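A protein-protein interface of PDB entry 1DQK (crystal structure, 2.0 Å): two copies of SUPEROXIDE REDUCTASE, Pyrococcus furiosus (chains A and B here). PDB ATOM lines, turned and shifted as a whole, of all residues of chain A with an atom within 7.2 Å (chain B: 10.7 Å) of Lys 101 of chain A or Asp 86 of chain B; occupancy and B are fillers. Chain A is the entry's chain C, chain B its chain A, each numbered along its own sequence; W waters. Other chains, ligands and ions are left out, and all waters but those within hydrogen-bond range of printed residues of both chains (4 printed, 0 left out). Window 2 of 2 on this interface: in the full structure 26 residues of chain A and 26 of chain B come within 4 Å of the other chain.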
ATOM      1  N   ARG A  24      -5.500  21.570   0.023  1.00  0.00           N
ATOM      2  CA  ARG A  24      -4.381  21.158  -0.814  1.00  0.00           C
ATOM      3  C   ARG A  24      -3.176  20.766   0.046  1.00  0.00           C
ATOM      4  O   ARG A  24      -2.713  21.546   0.878  1.00  0.00           O
ATOM      5  CB  ARG A  24      -4.003  22.297  -1.770  1.00  0.00           C
ATOM      6  CG  ARG A  24      -3.024  21.908  -2.877  1.00  0.00           C
ATOM      7  CD  ARG A  24      -3.285  22.694  -4.170  1.00  0.00           C
ATOM      8  NE  ARG A  24      -2.938  21.905  -5.348  1.00  0.00           N
ATOM      9  CZ  ARG A  24      -3.366  22.149  -6.584  1.00  0.00           C
ATOM     10  NH1 ARG A  24      -4.171  23.177  -6.826  1.00  0.00           N
ATOM     11  NH2 ARG A  24      -2.991  21.357  -7.580  1.00  0.00           N
ATOM     12  N   GLU A  27       0.765  17.401  -3.820  1.00  0.00           N
ATOM     13  CA  GLU A  27       0.134  17.154  -5.114  1.00  0.00           C
ATOM     14  C   GLU A  27      -1.247  16.566  -4.842  1.00  0.00           C
ATOM     15  O   GLU A  27      -1.982  16.200  -5.764  1.00  0.00           O
ATOM     16  CB  GLU A  27       0.962  16.158  -5.926  1.00  0.00           C
ATOM     17  CG  GLU A  27       1.222  14.845  -5.205  1.00  0.00           C
ATOM     18  CD  GLU A  27       2.473  14.142  -5.702  1.00  0.00           C
ATOM     19  OE1 GLU A  27       2.372  12.969  -6.118  1.00  0.00           O
ATOM     20  OE2 GLU A  27       3.556  14.764  -5.677  1.00  0.00           O
ATOM     21  N   VAL A  29      -5.061  16.891  -3.428  1.00  0.00           N
ATOM     22  CA  VAL A  29      -6.151  17.824  -3.184  1.00  0.00           C
ATOM     23  C   VAL A  29      -7.311  17.028  -2.598  1.00  0.00           C
ATOM     24  O   VAL A  29      -7.905  16.191  -3.282  1.00  0.00           O
ATOM     25  CB  VAL A  29      -6.634  18.505  -4.481  1.00  0.00           C
ATOM     26  CG1 VAL A  29      -7.827  19.397  -4.179  1.00  0.00           C
ATOM     27  CG2 VAL A  29      -5.505  19.318  -5.099  1.00  0.00           C
ATOM     28  N   PHE A  56     -13.615  18.345 -12.695  1.00  0.00           N
ATOM     29  CA  PHE A  56     -12.501  19.282 -12.649  1.00  0.00           C
ATOM     30  C   PHE A  56     -12.092  19.711 -14.056  1.00  0.00           C
ATOM     31  O   PHE A  56     -11.732  18.875 -14.892  1.00  0.00           O
ATOM     32  CB  PHE A  56     -11.304  18.638 -11.937  1.00  0.00           C
ATOM     33  CG  PHE A  56     -10.032  19.461 -11.987  1.00  0.00           C
ATOM     34  CD1 PHE A  56     -10.051  20.828 -11.727  1.00  0.00           C
ATOM     35  CD2 PHE A  56      -8.805  18.850 -12.250  1.00  0.00           C
ATOM     36  CE1 PHE A  56      -8.863  21.579 -11.722  1.00  0.00           C
ATOM     37  CE2 PHE A  56      -7.612  19.588 -12.247  1.00  0.00           C
ATOM     38  CZ  PHE A  56      -7.643  20.954 -11.981  1.00  0.00           C
ATOM     39  N   PRO A  58      -9.337  21.795 -15.747  1.00  0.00           N
ATOM     40  CA  PRO A  58      -8.078  22.505 -15.508  1.00  0.00           C
ATOM     41  C   PRO A  58      -8.053  23.859 -16.213  1.00  0.00           C
ATOM     42  O   PRO A  58      -8.646  24.030 -17.276  1.00  0.00           O
ATOM     43  CB  PRO A  58      -7.009  21.550 -16.043  1.00  0.00           C
ATOM     44  CG  PRO A  58      -7.692  20.195 -16.107  1.00  0.00           C
ATOM     45  CD  PRO A  58      -9.125  20.508 -16.435  1.00  0.00           C
ATOM     46  N   GLU A  59      -7.366  24.818 -15.608  1.00  0.00           N
ATOM     47  CA  GLU A  59      -7.256  26.160 -16.174  1.00  0.00           C
ATOM     48  C   GLU A  59      -6.735  26.156 -17.610  1.00  0.00           C
ATOM     49  O   GLU A  59      -5.672  25.601 -17.889  1.00  0.00           O
ATOM     50  CB  GLU A  59      -6.322  27.009 -15.308  1.00  0.00           C
ATOM     51  CG  GLU A  59      -6.215  28.460 -15.742  1.00  0.00           C
ATOM     52  CD  GLU A  59      -5.674  29.351 -14.642  1.00  0.00           C
ATOM     53  OE1 GLU A  59      -4.649  28.986 -14.031  1.00  0.00           O
ATOM     54  OE2 GLU A  59      -6.275  30.416 -14.391  1.00  0.00           O
ATOM     55  N   GLU A  61      -7.881  24.576 -20.226  1.00  0.00           N
ATOM     56  CA  GLU A  61      -8.134  23.369 -21.009  1.00  0.00           C
ATOM     57  C   GLU A  61      -9.567  23.316 -21.531  1.00  0.00           C
ATOM     58  O   GLU A  61     -10.441  24.012 -21.017  1.00  0.00           O
ATOM     59  CB  GLU A  61      -7.797  22.136 -20.170  1.00  0.00           C
ATOM     60  CG  GLU A  61      -6.320  22.082 -19.789  1.00  0.00           C
ATOM     61  CD  GLU A  61      -5.907  20.754 -19.185  1.00  0.00           C
ATOM     62  OE1 GLU A  61      -6.734  19.816 -19.191  1.00  0.00           O
ATOM     63  OE2 GLU A  61      -4.754  20.650 -18.702  1.00  0.00           O
ATOM     64  N   TYR A  65     -12.892  16.849 -16.649  1.00  0.00           N
ATOM     65  CA  TYR A  65     -12.660  15.465 -16.237  1.00  0.00           C
ATOM     66  C   TYR A  65     -13.565  15.145 -15.060  1.00  0.00           C
ATOM     67  O   TYR A  65     -13.744  15.972 -14.167  1.00  0.00           O
ATOM     68  CB  TYR A  65     -11.208  15.250 -15.791  1.00  0.00           C
ATOM     69  CG  TYR A  65     -10.185  15.388 -16.892  1.00  0.00           C
ATOM     70  CD1 TYR A  65      -9.268  16.438 -16.887  1.00  0.00           C
ATOM     71  CD2 TYR A  65     -10.144  14.479 -17.953  1.00  0.00           C
ATOM     72  CE1 TYR A  65      -8.339  16.588 -17.910  1.00  0.00           C
ATOM     73  CE2 TYR A  65      -9.220  14.618 -18.977  1.00  0.00           C
ATOM     74  CZ  TYR A  65      -8.322  15.677 -18.953  1.00  0.00           C
ATOM     75  OH  TYR A  65      -7.430  15.841 -19.992  1.00  0.00           O
ATOM     76  N   LEU A  97      -7.943  13.809  -4.763  1.00  0.00           N
ATOM     77  CA  LEU A  97      -7.447  14.049  -6.115  1.00  0.00           C
ATOM     78  C   LEU A  97      -5.946  14.338  -6.145  1.00  0.00           C
ATOM     79  O   LEU A  97      -5.441  15.157  -5.373  1.00  0.00           O
ATOM     80  CB  LEU A  97      -8.219  15.228  -6.719  1.00  0.00           C
ATOM     81  CG  LEU A  97      -7.753  15.894  -8.016  1.00  0.00           C
ATOM     82  CD1 LEU A  97      -8.135  15.032  -9.215  1.00  0.00           C
ATOM     83  CD2 LEU A  97      -8.403  17.261  -8.135  1.00  0.00           C
ATOM     84  N   LYS A  98      -5.233  13.660  -7.036  1.00  0.00           N
ATOM     85  CA  LYS A  98      -3.799  13.879  -7.172  1.00  0.00           C
ATOM     86  C   LYS A  98      -3.557  14.695  -8.433  1.00  0.00           C
ATOM     87  O   LYS A  98      -3.731  14.196  -9.547  1.00  0.00           O
ATOM     88  CB  LYS A  98      -3.053  12.546  -7.265  1.00  0.00           C
ATOM     89  CG  LYS A  98      -1.541  12.681  -7.258  1.00  0.00           C
ATOM     90  CD  LYS A  98      -0.884  11.456  -6.643  1.00  0.00           C
ATOM     91  CE  LYS A  98      -0.132  10.650  -7.688  1.00  0.00           C
ATOM     92  NZ  LYS A  98      -1.051  10.031  -8.686  1.00  0.00           N
ATOM     93  N   THR A  99      -3.186  15.958  -8.250  1.00  0.00           N
ATOM     94  CA  THR A  99      -2.906  16.856  -9.367  1.00  0.00           C
ATOM     95  C   THR A  99      -2.163  18.103  -8.896  1.00  0.00           C
ATOM     96  O   THR A  99      -2.283  18.512  -7.737  1.00  0.00           O
ATOM     97  CB  THR A  99      -4.196  17.323 -10.064  1.00  0.00           C
ATOM     98  OG1 THR A  99      -3.855  18.080 -11.234  1.00  0.00           O
ATOM     99  CG2 THR A  99      -5.027  18.200  -9.133  1.00  0.00           C
ATOM    100  N   LYS A 100      -1.402  18.704  -9.805  1.00  0.00           N
ATOM    101  CA  LYS A 100      -0.650  19.915  -9.499  1.00  0.00           C
ATOM    102  C   LYS A 100      -1.240  21.064 -10.308  1.00  0.00           C
ATOM    103  O   LYS A 100      -0.773  22.202 -10.241  1.00  0.00           O
ATOM    104  CB  LYS A 100       0.825  19.731  -9.862  1.00  0.00           C
ATOM    105  CG  LYS A 100       1.593  18.842  -8.898  1.00  0.00           C
ATOM    106  CD  LYS A 100       3.076  19.174  -8.902  1.00  0.00           C
ATOM    107  CE  LYS A 100       3.870  18.156  -8.102  1.00  0.00           C
ATOM    108  NZ  LYS A 100       4.428  18.745  -6.852  1.00  0.00           N
ATOM    109  N   LYS A 101      -2.286  20.761 -11.068  1.00  0.00           N
ATOM    110  CA  LYS A 101      -2.927  21.771 -11.892  1.00  0.00           C
ATOM    111  C   LYS A 101      -3.925  22.578 -11.082  1.00  0.00           C
ATOM    112  O   LYS A 101      -4.302  22.203  -9.968  1.00  0.00           O
ATOM    113  CB  LYS A 101      -3.643  21.114 -13.079  1.00  0.00           C
ATOM    114  CG  LYS A 101      -2.711  20.574 -14.164  1.00  0.00           C
ATOM    115  CD  LYS A 101      -3.503  19.845 -15.239  1.00  0.00           C
ATOM    116  CE  LYS A 101      -2.606  19.308 -16.350  1.00  0.00           C
ATOM    117  NZ  LYS A 101      -3.425  18.701 -17.459  1.00  0.00           N
ATOM    118  N   LYS A 102      -4.343  23.699 -11.652  1.00  0.00           N
ATOM    119  CA  LYS A 102      -5.323  24.565 -11.017  1.00  0.00           C
ATOM    120  C   LYS A 102      -6.492  24.623 -11.977  1.00  0.00           C
ATOM    121  O   LYS A 102      -6.372  24.189 -13.124  1.00  0.00           O
ATOM    122  CB  LYS A 102      -4.757  25.971 -10.818  1.00  0.00           C
ATOM    123  CG  LYS A 102      -3.506  26.024  -9.960  1.00  0.00           C
ATOM    124  CD  LYS A 102      -3.075  27.465  -9.733  1.00  0.00           C
ATOM    125  CE  LYS A 102      -1.723  27.536  -9.042  1.00  0.00           C
ATOM    126  NZ  LYS A 102      -0.862  28.585  -9.650  1.00  0.00           N
ATOM    127  N   GLY A 103      -7.619  25.147 -11.517  1.00  0.00           N
ATOM    128  CA  GLY A 103      -8.771  25.240 -12.390  1.00  0.00           C
ATOM    129  C   GLY A 103     -10.073  25.437 -11.645  1.00  0.00           C
ATOM    130  O   GLY A 103     -10.129  26.142 -10.638  1.00  0.00           O
ATOM    131  N   LEU A 123     -10.231  26.126  -7.955  1.00  0.00           N
ATOM    132  CA  LEU A 123      -9.201  25.345  -7.285  1.00  0.00           C
ATOM    133  C   LEU A 123      -7.898  26.115  -7.465  1.00  0.00           C
ATOM    134  O   LEU A 123      -7.326  26.139  -8.558  1.00  0.00           O
ATOM    135  CB  LEU A 123      -9.073  23.951  -7.911  1.00  0.00           C
ATOM    136  CG  LEU A 123      -7.868  23.110  -7.461  1.00  0.00           C
ATOM    137  CD1 LEU A 123      -7.750  23.129  -5.946  1.00  0.00           C
ATOM    138  CD2 LEU A 123      -8.029  21.681  -7.950  1.00  0.00           C
ATOM    139  N   GLU A 124      -7.441  26.757  -6.395  1.00  0.00           N
ATOM    140  CA  GLU A 124      -6.217  27.540  -6.452  1.00  0.00           C
ATOM    141  C   GLU A 124      -4.977  26.662  -6.371  1.00  0.00           C
ATOM    142  O   GLU A 124      -5.060  25.564  -5.783  1.00  0.00           O
ATOM    143  CB  GLU A 124      -6.205  28.570  -5.322  1.00  0.00           C
ATOM    144  CG  GLU A 124      -7.028  29.813  -5.623  1.00  0.00           C
ATOM    145  CD  GLU A 124      -7.273  30.668  -4.390  1.00  0.00           C
ATOM    146  OE1 GLU A 124      -8.448  30.973  -4.102  1.00  0.00           O
ATOM    147  OE2 GLU A 124      -6.291  31.034  -3.708  1.00  0.00           O
ATOM    148  OXT GLU A 124      -3.933  27.088  -6.904  1.00  0.00           O
ATOM    149  N   ASN B  43      -1.909   3.706 -10.280  1.00  0.00           N
ATOM    150  CA  ASN B  43      -3.057   4.484 -10.724  1.00  0.00           C
ATOM    151  C   ASN B  43      -2.653   5.123 -12.028  1.00  0.00           C
ATOM    152  O   ASN B  43      -2.256   6.291 -12.079  1.00  0.00           O
ATOM    153  CB  ASN B  43      -3.463   5.568  -9.717  1.00  0.00           C
ATOM    154  CG  ASN B  43      -4.797   6.220 -10.078  1.00  0.00           C
ATOM    155  OD1 ASN B  43      -5.382   5.923 -11.125  1.00  0.00           O
ATOM    156  ND2 ASN B  43      -5.280   7.112  -9.217  1.00  0.00           N
ATOM    157  N   THR B  44      -2.739   4.328 -13.086  1.00  0.00           N
ATOM    158  CA  THR B  44      -2.384   4.780 -14.416  1.00  0.00           C
ATOM    159  C   THR B  44      -3.563   4.513 -15.322  1.00  0.00           C
ATOM    160  O   THR B  44      -4.503   3.804 -14.947  1.00  0.00           O
ATOM    161  CB  THR B  44      -1.166   4.007 -14.962  1.00  0.00           C
ATOM    162  OG1 THR B  44      -1.528   2.633 -15.173  1.00  0.00           O
ATOM    163  CG2 THR B  44      -0.006   4.075 -13.977  1.00  0.00           C
ATOM    164  N   THR B  45      -3.505   5.067 -16.523  1.00  0.00           N
ATOM    165  CA  THR B  45      -4.570   4.879 -17.487  1.00  0.00           C
ATOM    166  C   THR B  45      -4.795   3.389 -17.767  1.00  0.00           C
ATOM    167  O   THR B  45      -5.936   2.940 -17.930  1.00  0.00           O
ATOM    168  CB  THR B  45      -4.243   5.608 -18.806  1.00  0.00           C
ATOM    169  OG1 THR B  45      -4.096   7.012 -18.551  1.00  0.00           O
ATOM    170  CG2 THR B  45      -5.357   5.409 -19.816  1.00  0.00           C
ATOM    171  N   ALA B  74     -10.834   9.415 -12.574  1.00  0.00           N
ATOM    172  CA  ALA B  74      -9.753  10.047 -13.323  1.00  0.00           C
ATOM    173  C   ALA B  74      -8.484   9.220 -13.205  1.00  0.00           C
ATOM    174  O   ALA B  74      -8.056   8.894 -12.099  1.00  0.00           O
ATOM    175  CB  ALA B  74      -9.493  11.463 -12.808  1.00  0.00           C
ATOM    176  N   HIS B  75      -7.871   8.889 -14.337  1.00  0.00           N
ATOM    177  CA  HIS B  75      -6.647   8.098 -14.301  1.00  0.00           C
ATOM    178  C   HIS B  75      -5.542   8.547 -15.256  1.00  0.00           C
ATOM    179  O   HIS B  75      -4.829   7.723 -15.823  1.00  0.00           O
ATOM    180  CB  HIS B  75      -6.988   6.624 -14.523  1.00  0.00           C
ATOM    181  CG  HIS B  75      -8.122   6.149 -13.671  1.00  0.00           C
ATOM    182  ND1 HIS B  75      -7.982   5.899 -12.322  1.00  0.00           N
ATOM    183  CD2 HIS B  75      -9.428   5.943 -13.960  1.00  0.00           C
ATOM    184  CE1 HIS B  75      -9.155   5.560 -11.816  1.00  0.00           C
ATOM    185  NE2 HIS B  75     -10.049   5.579 -12.790  1.00  0.00           N
ATOM    186  N   GLY B  76      -5.400   9.863 -15.415  1.00  0.00           N
ATOM    187  CA  GLY B  76      -4.350  10.421 -16.256  1.00  0.00           C
ATOM    188  C   GLY B  76      -4.600  10.536 -17.745  1.00  0.00           C
ATOM    189  O   GLY B  76      -3.820  11.167 -18.463  1.00  0.00           O
ATOM    190  N   GLU B  77      -5.680   9.934 -18.225  1.00  0.00           N
ATOM    191  CA  GLU B  77      -5.996   9.976 -19.646  1.00  0.00           C
ATOM    192  C   GLU B  77      -6.314  11.393 -20.160  1.00  0.00           C
ATOM    193  O   GLU B  77      -6.973  12.178 -19.479  1.00  0.00           O
ATOM    194  CB  GLU B  77      -7.182   9.050 -19.926  1.00  0.00           C
ATOM    195  CG  GLU B  77      -8.471   9.436 -19.183  1.00  0.00           C
ATOM    196  CD  GLU B  77      -8.459   9.034 -17.718  1.00  0.00           C
ATOM    197  OE1 GLU B  77      -7.777   8.042 -17.374  1.00  0.00           O
ATOM    198  OE2 GLU B  77      -9.140   9.713 -16.908  1.00  0.00           O
ATOM    199  N   SER B  78      -5.838  11.710 -21.364  1.00  0.00           N
ATOM    200  CA  SER B  78      -6.107  13.004 -21.983  1.00  0.00           C
ATOM    201  C   SER B  78      -5.926  12.905 -23.498  1.00  0.00           C
ATOM    202  O   SER B  78      -5.454  11.890 -24.004  1.00  0.00           O
ATOM    203  CB  SER B  78      -5.184  14.088 -21.405  1.00  0.00           C
ATOM    204  OG  SER B  78      -4.037  14.287 -22.216  1.00  0.00           O
ATOM    205  N   VAL B  79      -6.307  13.955 -24.224  1.00  0.00           N
ATOM    206  CA  VAL B  79      -6.165  13.945 -25.678  1.00  0.00           C
ATOM    207  C   VAL B  79      -4.699  13.819 -26.089  1.00  0.00           C
ATOM    208  O   VAL B  79      -4.395  13.504 -27.239  1.00  0.00           O
ATOM    209  CB  VAL B  79      -6.744  15.231 -26.319  1.00  0.00           C
ATOM    210  CG1 VAL B  79      -8.262  15.222 -26.220  1.00  0.00           C
ATOM    211  CG2 VAL B  79      -6.178  16.460 -25.637  1.00  0.00           C
ATOM    212  N   ASN B  80      -3.796  14.053 -25.138  1.00  0.00           N
ATOM    213  CA  ASN B  80      -2.368  13.967 -25.404  1.00  0.00           C
ATOM    214  C   ASN B  80      -1.813  12.584 -25.100  1.00  0.00           C
ATOM    215  O   ASN B  80      -0.596  12.388 -25.099  1.00  0.00           O
ATOM    216  CB  ASN B  80      -1.612  15.024 -24.588  1.00  0.00           C
ATOM    217  CG  ASN B  80      -1.692  16.401 -25.217  1.00  0.00           C
ATOM    218  OD1 ASN B  80      -2.050  16.534 -26.385  1.00  0.00           O
ATOM    219  ND2 ASN B  80      -1.364  17.430 -24.450  1.00  0.00           N
ATOM    220  N   GLY B  81      -2.710  11.633 -24.826  1.00  0.00           N
ATOM    221  CA  GLY B  81      -2.282  10.274 -24.548  1.00  0.00           C
ATOM    222  C   GLY B  81      -2.496   9.800 -23.122  1.00  0.00           C
ATOM    223  O   GLY B  81      -2.895  10.579 -22.258  1.00  0.00           O
ATOM    224  N   PRO B  82      -2.229   8.515 -22.845  1.00  0.00           N
ATOM    225  CA  PRO B  82      -2.400   7.961 -21.496  1.00  0.00           C
ATOM    226  C   PRO B  82      -1.427   8.615 -20.510  1.00  0.00           C
ATOM    227  O   PRO B  82      -0.316   8.989 -20.884  1.00  0.00           O
ATOM    228  CB  PRO B  82      -2.105   6.466 -21.680  1.00  0.00           C
ATOM    229  CG  PRO B  82      -1.230   6.404 -22.896  1.00  0.00           C
ATOM    230  CD  PRO B  82      -1.726   7.508 -23.796  1.00  0.00           C
ATOM    231  N   ASN B  83      -1.861   8.765 -19.262  1.00  0.00           N
ATOM    232  CA  ASN B  83      -1.031   9.346 -18.208  1.00  0.00           C
ATOM    233  C   ASN B  83      -0.432  10.715 -18.535  1.00  0.00           C
ATOM    234  O   ASN B  83       0.750  10.947 -18.276  1.00  0.00           O
ATOM    235  CB  ASN B  83       0.112   8.389 -17.864  1.00  0.00           C
ATOM    236  CG  ASN B  83      -0.363   6.971 -17.636  1.00  0.00           C
ATOM    237  OD1 ASN B  83       0.073   6.039 -18.316  1.00  0.00           O
ATOM    238  ND2 ASN B  83      -1.263   6.796 -16.672  1.00  0.00           N
ATOM    239  N   THR B  84      -1.232  11.625 -19.079  1.00  0.00           N
ATOM    240  CA  THR B  84      -0.714  12.948 -19.420  1.00  0.00           C
ATOM    241  C   THR B  84      -1.543  14.100 -18.857  1.00  0.00           C
ATOM    242  O   THR B  84      -1.141  15.262 -18.968  1.00  0.00           O
ATOM    243  CB  THR B  84      -0.640  13.137 -20.949  1.00  0.00           C
ATOM    244  OG1 THR B  84      -1.927  12.874 -21.530  1.00  0.00           O
ATOM    245  CG2 THR B  84       0.396  12.195 -21.556  1.00  0.00           C
ATOM    246  N   SER B  85      -2.685  13.787 -18.251  1.00  0.00           N
ATOM    247  CA  SER B  85      -3.563  14.826 -17.718  1.00  0.00           C
ATOM    248  C   SER B  85      -3.157  15.388 -16.367  1.00  0.00           C
ATOM    249  O   SER B  85      -3.594  16.473 -15.999  1.00  0.00           O
ATOM    250  CB  SER B  85      -4.996  14.300 -17.608  1.00  0.00           C
ATOM    251  OG  SER B  85      -5.171  13.593 -16.391  1.00  0.00           O
ATOM    252  N   ASP B  86      -2.326  14.658 -15.635  1.00  0.00           N
ATOM    253  CA  ASP B  86      -1.915  15.072 -14.294  1.00  0.00           C
ATOM    254  C   ASP B  86      -3.137  15.121 -13.361  1.00  0.00           C
ATOM    255  O   ASP B  86      -3.130  15.815 -12.340  1.00  0.00           O
ATOM    256  CB  ASP B  86      -1.223  16.443 -14.312  1.00  0.00           C
ATOM    257  CG  ASP B  86      -0.570  16.780 -12.977  1.00  0.00           C
ATOM    258  OD1 ASP B  86      -0.694  17.935 -12.514  1.00  0.00           O
ATOM    259  OD2 ASP B  86       0.062  15.886 -12.378  1.00  0.00           O
ATOM    260  N   VAL B  87      -4.184  14.387 -13.721  1.00  0.00           N
ATOM    261  CA  VAL B  87      -5.400  14.318 -12.902  1.00  0.00           C
ATOM    262  C   VAL B  87      -5.693  12.850 -12.566  1.00  0.00           C
ATOM    263  O   VAL B  87      -6.083  12.067 -13.443  1.00  0.00           O
ATOM    264  CB  VAL B  87      -6.630  14.902 -13.638  1.00  0.00           C
ATOM    265  CG1 VAL B  87      -7.854  14.833 -12.728  1.00  0.00           C
ATOM    266  CG2 VAL B  87      -6.362  16.345 -14.063  1.00  0.00           C
ATOM    267  N   TYR B  88      -5.509  12.480 -11.301  1.00  0.00           N
ATOM    268  CA  TYR B  88      -5.743  11.101 -10.864  1.00  0.00           C
ATOM    269  C   TYR B  88      -6.586  11.053  -9.600  1.00  0.00           C
ATOM    270  O   TYR B  88      -6.368  11.836  -8.677  1.00  0.00           O
ATOM    271  CB  TYR B  88      -4.412  10.396 -10.575  1.00  0.00           C
ATOM    272  CG  TYR B  88      -3.485  10.304 -11.760  1.00  0.00           C
ATOM    273  CD1 TYR B  88      -2.670  11.375 -12.110  1.00  0.00           C
ATOM    274  CD2 TYR B  88      -3.432   9.147 -12.539  1.00  0.00           C
ATOM    275  CE1 TYR B  88      -1.822  11.305 -13.206  1.00  0.00           C
ATOM    276  CE2 TYR B  88      -2.590   9.063 -13.639  1.00  0.00           C
ATOM    277  CZ  TYR B  88      -1.786  10.148 -13.968  1.00  0.00           C
ATOM    278  OH  TYR B  88      -0.951  10.079 -15.059  1.00  0.00           O
ATOM    279  N   THR B  89      -7.537  10.126  -9.550  1.00  0.00           N
ATOM    280  CA  THR B  89      -8.390   9.986  -8.371  1.00  0.00           C
ATOM    281  C   THR B  89      -7.911   8.783  -7.569  1.00  0.00           C
ATOM    282  O   THR B  89      -7.979   7.642  -8.037  1.00  0.00           O
ATOM    283  CB  THR B  89      -9.867   9.788  -8.764  1.00  0.00           C
ATOM    284  OG1 THR B  89     -10.246  10.816  -9.685  1.00  0.00           O
ATOM    285  CG2 THR B  89     -10.774   9.873  -7.532  1.00  0.00           C
ATOM    286  N   GLU B  90      -7.416   9.048  -6.366  1.00  0.00           N
ATOM    287  CA  GLU B  90      -6.898   7.997  -5.499  1.00  0.00           C
ATOM    288  C   GLU B  90      -8.014   7.135  -4.920  1.00  0.00           C
ATOM    289  O   GLU B  90      -9.089   7.637  -4.568  1.00  0.00           O
ATOM    290  CB  GLU B  90      -6.068   8.615  -4.366  1.00  0.00           C
ATOM    291  CG  GLU B  90      -4.774   9.264  -4.842  1.00  0.00           C
ATOM    292  CD  GLU B  90      -3.871   8.285  -5.563  1.00  0.00           C
ATOM    293  OE1 GLU B  90      -3.167   7.516  -4.878  1.00  0.00           O
ATOM    294  OE2 GLU B  90      -3.872   8.278  -6.814  1.00  0.00           O
HETATM  295  O   HOH W   1      -8.376  15.504 -22.461  1.00  0.00           O
HETATM  296  O   HOH W   2      -2.416  17.467 -19.993  1.00  0.00           O
HETATM  297  O   HOH W   3      -0.932   7.069  -7.101  1.00  0.00           O
HETATM  298  O   HOH W   4      -1.002  13.994 -10.646  1.00  0.00           O
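CG2 of Val 87 of chain B touches CE2 of Phe 56 of chain A, at 3.9 Å. CE2 of Tyr 65 of chain A touches O of Glu 77 of chain B (3.4 Å). Tyr 65 of chain A touches Ser 78 of chain B. Ser 85 of chain B touches Tyr 65 of chain A. CG1 of Val 87 of chain B touches CD1 of Leu 97 of chain A (3.5 Å). Tyr 88 of chain B touches Leu 97 of chain A. Lys 98 of chain A touches Val 87 of chain B (O to CA, 3.7 Å). OD1 of Asp 86 of chain B touches N of Lys 101 of chain A (3.6 Å).
Hydrophobic or aromatic side chains of chain A that line the printed part of chain B: Phe 56, Tyr 65 and Leu 97. Of the 20 printed residues of chain B, 7 touch a printed residue of chain A. Along chain B the printed residues that touch a printed residue of chain A span positions 77 to 90. Among the printed residues, 14 pairs touch across the chains. Among the printed residues, Asp or Glu carboxylates within 4 Å of a Lys or Arg side-chain nitrogen of the other chain: Lys 98 of chain A with Glu 90 of chain B.
Water W1 lies within hydrogen-bond range of OH of Tyr 65 of chain A (2.7 Å) and N of Val 79 of chain B (3.1 Å). Water W2 bridges O of Thr 84 of chain B (2.7 Å) and NZ of Lys 101 of chain A (3.0 Å). Water W4 lies within hydrogen-bond range of the side-chain carboxylate of Asp 86 of chain B and the backbone carbonyl oxygen of Lys 98 of chain A. Water W3 bridges the side-chain carboxylate (OE1) of Glu 90 of chain B (3.2 Å) and the side-chain amino group (NZ) of Lys 98 of chain A (3.4 Å).
The side-chain amino group of Lys 101 of chain A lies within hydrogen-bond range of the backbone carbonyl oxygen of Ser 85 of chain B (2.7 Å). The side-chain hydroxyl (OG1) of Thr 99 of chain A lies within hydrogen-bond range of the backbone carbonyl oxygen (O) of Asp 86 of chain B (2.6 Å). OD1 of Asp 86 of chain B is in hydrogen-bond range of N of Lys 100 of chain A. The backbone NH (N) of Lys 98 of chain A is in hydrogen-bond range of the backbone carbonyl oxygen (O) of Tyr 88 of chain B (2.7 Å). NZ of Lys 98 of chain A is in salt-bridge range of OE2 of Glu 90 of chain B (3.8 Å). The backbone carbonyl oxygen (O) of Lys 98 of chain A lies close to the backbone carbonyl oxygen (O) of Asp 86 of chain B, at 3.3 Å.
The side-chain amide nitrogen (ND2) of Asn 43 of chain B lies within hydrogen-bond range of the side-chain carboxylate (OE2) of Glu 90 of chain B (3.0 Å). The backbone NH (N) of Glu 77 of chain B sits at hydrogen-bond distance from the side-chain hydroxyl (OG1) of Thr 45 of chain B, at 3.3 Å. The backbone carbonyl oxygen (O) of Gly 76 of chain B is in hydrogen-bond range of the backbone NH (N) of Ser 85 of chain B (2.9 Å). OG of Ser 78 of chain B sits close to N of Asn 80 of chain B. O of Thr 99 of chain A lies within hydrogen-bond range of NH2 of Arg 24 of chain A. The backbone carbonyl oxygen of Glu 27 of chain A is in hydrogen-bond range of the backbone NH of Thr 99 of chain A, 2.8 Å away.
No position is printed for both chains. Of the 14 pairs that touch across the chains among the printed residues, none has its exchanged pair printed and touching as well.
Of chain B, only Ser 85 and Asp 86 come within 4 Å of Lys 101 of chain A. Asp 86 of chain B touches just these residues of chain A: Lys 98 (3.3 Å), Thr 99 (2.6 Å), Lys 100 (2.9 Å) and Lys 101 (3.6 Å). Of chain B, only Asp 86 (2.6 Å) comes within 4 Å of Thr 99 of chain A. Of the printed residues of chain A, Val 87 of chain B touches Phe 56 (3.9 Å), Leu 97 (3.5 Å) and Lys 98 (3.7 Å). Of the printed residues of chain A, Glu 90 of chain B touches Lys 98. Of the printed residues of chain A, Ser 78 of chain B touches Tyr 65 (3.2 Å). The nearest residue of chain B that does not touch Lys 101 of chain A is Thr 84 of chain B (4.4 Å). The nearest printed residue of chain B that does not touch Leu 97 of chain A is Thr 89 of chain B (4.7 Å).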
